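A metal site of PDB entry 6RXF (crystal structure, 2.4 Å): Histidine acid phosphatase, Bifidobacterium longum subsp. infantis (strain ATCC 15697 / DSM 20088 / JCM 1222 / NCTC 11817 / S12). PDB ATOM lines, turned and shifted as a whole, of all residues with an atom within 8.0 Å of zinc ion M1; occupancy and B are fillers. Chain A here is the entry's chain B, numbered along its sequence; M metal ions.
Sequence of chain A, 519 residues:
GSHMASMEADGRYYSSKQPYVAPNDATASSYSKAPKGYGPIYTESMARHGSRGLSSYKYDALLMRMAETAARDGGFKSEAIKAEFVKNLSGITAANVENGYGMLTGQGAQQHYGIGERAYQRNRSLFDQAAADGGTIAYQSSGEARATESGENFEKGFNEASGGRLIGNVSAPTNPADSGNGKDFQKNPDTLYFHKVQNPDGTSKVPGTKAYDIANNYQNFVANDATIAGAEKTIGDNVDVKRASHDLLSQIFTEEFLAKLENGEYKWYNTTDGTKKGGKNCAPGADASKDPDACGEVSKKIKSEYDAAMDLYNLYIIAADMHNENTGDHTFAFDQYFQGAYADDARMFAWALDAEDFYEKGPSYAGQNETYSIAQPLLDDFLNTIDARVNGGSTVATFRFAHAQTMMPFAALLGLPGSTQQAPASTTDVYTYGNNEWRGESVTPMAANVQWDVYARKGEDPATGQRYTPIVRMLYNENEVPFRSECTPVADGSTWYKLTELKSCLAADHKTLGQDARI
Zinc ion M1 is bound by OE2 of Glu 356.
Zinc ion M1 is bound by OE2 of Glu 360.
OE2 of Glu 232 is bound to zinc ion M1, 2.4 Å away.
Slightly farther from zinc ion M1 lies the side-chain carboxylate (OE1) of Glu 232 (2.8 Å).
Three residues have an atom within 4 Å of zinc ion M1: Glu 232, Glu 356 and Glu 360.
The nearest printed residue that does not touch zinc ion M1 is Ile 228 (5.5 Å).
NZ of Lys 361 lies within salt-bridge range of OE1 of Glu 360.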
ATOM      1  N   VAL A 222     -18.866  -8.783  34.300  1.00  0.00           N
ATOM      2  CA  VAL A 222     -18.777  -7.826  33.199  1.00  0.00           C
ATOM      3  C   VAL A 222     -18.333  -8.511  31.914  1.00  0.00           C
ATOM      4  O   VAL A 222     -18.852  -8.216  30.829  1.00  0.00           O
ATOM      5  CB  VAL A 222     -17.838  -6.660  33.590  1.00  0.00           C
ATOM      6  CG1 VAL A 222     -17.272  -5.983  32.359  1.00  0.00           C
ATOM      7  CG2 VAL A 222     -18.605  -5.653  34.426  1.00  0.00           C
ATOM      8  N   ALA A 223     -17.392  -9.448  31.999  1.00  0.00           N
ATOM      9  CA  ALA A 223     -16.912 -10.126  30.797  1.00  0.00           C
ATOM     10  C   ALA A 223     -17.953 -11.055  30.194  1.00  0.00           C
ATOM     11  O   ALA A 223     -17.868 -11.357  28.992  1.00  0.00           O
ATOM     12  CB  ALA A 223     -15.631 -10.898  31.105  1.00  0.00           C
ATOM     13  N   ILE A 228     -25.426  -6.724  28.923  1.00  0.00           N
ATOM     14  CA  ILE A 228     -24.413  -5.718  28.604  1.00  0.00           C
ATOM     15  C   ILE A 228     -23.855  -5.961  27.210  1.00  0.00           C
ATOM     16  O   ILE A 228     -23.705  -5.022  26.413  1.00  0.00           O
ATOM     17  CB  ILE A 228     -23.300  -5.724  29.672  1.00  0.00           C
ATOM     18  CG1 ILE A 228     -23.831  -5.219  31.010  1.00  0.00           C
ATOM     19  CG2 ILE A 228     -22.121  -4.875  29.204  1.00  0.00           C
ATOM     20  CD1 ILE A 228     -22.894  -5.454  32.177  1.00  0.00           C
ATOM     21  N   ALA A 229     -23.540  -7.212  26.883  1.00  0.00           N
ATOM     22  CA  ALA A 229     -22.970  -7.536  25.587  1.00  0.00           C
ATOM     23  C   ALA A 229     -23.918  -7.160  24.451  1.00  0.00           C
ATOM     24  O   ALA A 229     -23.486  -6.635  23.422  1.00  0.00           O
ATOM     25  CB  ALA A 229     -22.630  -9.030  25.517  1.00  0.00           C
ATOM     26  N   GLU A 232     -24.219  -3.214  24.197  1.00  0.00           N
ATOM     27  CA  GLU A 232     -23.038  -2.611  23.593  1.00  0.00           C
ATOM     28  C   GLU A 232     -22.920  -2.949  22.112  1.00  0.00           C
ATOM     29  O   GLU A 232     -22.412  -2.149  21.322  1.00  0.00           O
ATOM     30  CB  GLU A 232     -21.780  -3.062  24.337  1.00  0.00           C
ATOM     31  CG  GLU A 232     -21.547  -2.308  25.661  1.00  0.00           C
ATOM     32  CD  GLU A 232     -20.138  -2.430  26.188  1.00  0.00           C
ATOM     33  OE1 GLU A 232     -19.406  -1.421  26.165  1.00  0.00           O
ATOM     34  OE2 GLU A 232     -19.767  -3.538  26.640  1.00  0.00           O
ATOM     35  N   LYS A 233     -23.375  -4.143  21.721  1.00  0.00           N
ATOM     36  CA  LYS A 233     -23.456  -4.458  20.302  1.00  0.00           C
ATOM     37  C   LYS A 233     -24.441  -3.531  19.596  1.00  0.00           C
ATOM     38  O   LYS A 233     -24.167  -3.052  18.490  1.00  0.00           O
ATOM     39  CB  LYS A 233     -23.867  -5.923  20.125  1.00  0.00           C
ATOM     40  CG  LYS A 233     -23.655  -6.468  18.728  1.00  0.00           C
ATOM     41  CD  LYS A 233     -24.974  -6.883  18.073  1.00  0.00           C
ATOM     42  CE  LYS A 233     -24.732  -7.651  16.775  1.00  0.00           C
ATOM     43  NZ  LYS A 233     -23.896  -6.871  15.805  1.00  0.00           N
ATOM     44  N   ALA A 355     -21.704   5.424  27.148  1.00  0.00           N
ATOM     45  CA  ALA A 355     -22.486   4.206  27.186  1.00  0.00           C
ATOM     46  C   ALA A 355     -21.701   3.039  27.775  1.00  0.00           C
ATOM     47  O   ALA A 355     -22.178   2.344  28.681  1.00  0.00           O
ATOM     48  CB  ALA A 355     -23.013   3.868  25.787  1.00  0.00           C
ATOM     49  N   GLU A 356     -20.472   2.815  27.275  1.00  0.00           N
ATOM     50  CA  GLU A 356     -19.639   1.725  27.789  1.00  0.00           C
ATOM     51  C   GLU A 356     -19.376   1.876  29.283  1.00  0.00           C
ATOM     52  O   GLU A 356     -19.455   0.913  30.056  1.00  0.00           O
ATOM     53  CB  GLU A 356     -18.313   1.665  27.024  1.00  0.00           C
ATOM     54  CG  GLU A 356     -17.287   0.736  27.684  1.00  0.00           C
ATOM     55  OE1 GLU A 356     -16.359   0.157  25.581  1.00  0.00           O
ATOM     56  OE2 GLU A 356     -16.517  -1.420  27.084  1.00  0.00           O
ATOM     57  N   ASP A 357     -19.011   3.099  29.674  1.00  0.00           N
ATOM     58  CA  ASP A 357     -18.814   3.403  31.088  1.00  0.00           C
ATOM     59  C   ASP A 357     -20.105   3.194  31.888  1.00  0.00           C
ATOM     60  O   ASP A 357     -20.072   2.606  32.979  1.00  0.00           O
ATOM     61  CB  ASP A 357     -18.309   4.834  31.241  1.00  0.00           C
ATOM     62  CG  ASP A 357     -16.793   4.922  31.213  1.00  0.00           C
ATOM     63  OD1 ASP A 357     -16.141   3.907  31.494  1.00  0.00           O
ATOM     64  OD2 ASP A 357     -16.251   6.026  30.946  1.00  0.00           O
ATOM     65  N   TYR A 359     -22.723   1.237  31.344  1.00  0.00           N
ATOM     66  CA  TYR A 359     -23.128  -0.152  31.488  1.00  0.00           C
ATOM     67  C   TYR A 359     -22.141  -0.979  32.303  1.00  0.00           C
ATOM     68  O   TYR A 359     -22.544  -2.014  32.852  1.00  0.00           O
ATOM     69  CB  TYR A 359     -23.292  -0.810  30.122  1.00  0.00           C
ATOM     70  CG  TYR A 359     -24.623  -0.534  29.457  1.00  0.00           C
ATOM     71  CD1 TYR A 359     -25.806  -1.054  29.979  1.00  0.00           C
ATOM     72  CD2 TYR A 359     -24.702   0.256  28.326  1.00  0.00           C
ATOM     73  CE1 TYR A 359     -27.020  -0.802  29.381  1.00  0.00           C
ATOM     74  CE2 TYR A 359     -25.902   0.518  27.717  1.00  0.00           C
ATOM     75  CZ  TYR A 359     -27.058  -0.011  28.249  1.00  0.00           C
ATOM     76  OH  TYR A 359     -28.255   0.255  27.627  1.00  0.00           O
ATOM     77  N   GLU A 360     -20.881  -0.562  32.413  1.00  0.00           N
ATOM     78  CA  GLU A 360     -19.877  -1.385  33.068  1.00  0.00           C
ATOM     79  C   GLU A 360     -19.524  -0.916  34.474  1.00  0.00           C
ATOM     80  O   GLU A 360     -19.187  -1.749  35.318  1.00  0.00           O
ATOM     81  CB  GLU A 360     -18.603  -1.437  32.215  1.00  0.00           C
ATOM     82  CG  GLU A 360     -18.796  -2.154  30.887  1.00  0.00           C
ATOM     83  CD  GLU A 360     -17.500  -2.313  30.119  1.00  0.00           C
ATOM     84  OE1 GLU A 360     -16.498  -1.674  30.500  1.00  0.00           O
ATOM     85  OE2 GLU A 360     -17.490  -3.088  29.137  1.00  0.00           O
ATOM     86  N   LYS A 361     -19.596   0.386  34.737  1.00  0.00           N
ATOM     87  CA  LYS A 361     -19.223   0.908  36.042  1.00  0.00           C
ATOM     88  C   LYS A 361     -20.291   1.768  36.688  1.00  0.00           C
ATOM     89  O   LYS A 361     -20.144   2.119  37.869  1.00  0.00           O
ATOM     90  CB  LYS A 361     -17.918   1.719  35.950  1.00  0.00           C
ATOM     91  CG  LYS A 361     -16.735   0.952  35.364  1.00  0.00           C
ATOM     92  CD  LYS A 361     -16.324   1.511  34.006  1.00  0.00           C
ATOM     93  CE  LYS A 361     -15.146   0.742  33.412  1.00  0.00           C
ATOM     94  NZ  LYS A 361     -15.529  -0.614  32.913  1.00  0.00           N
HETATM   95 ZN    ZN M   1     -17.355  -3.265  26.870  1.00  0.00          ZN
HETATM   96 ZN    ZN M   2     -18.407  -6.287  26.787  1.00  0.00          ZN
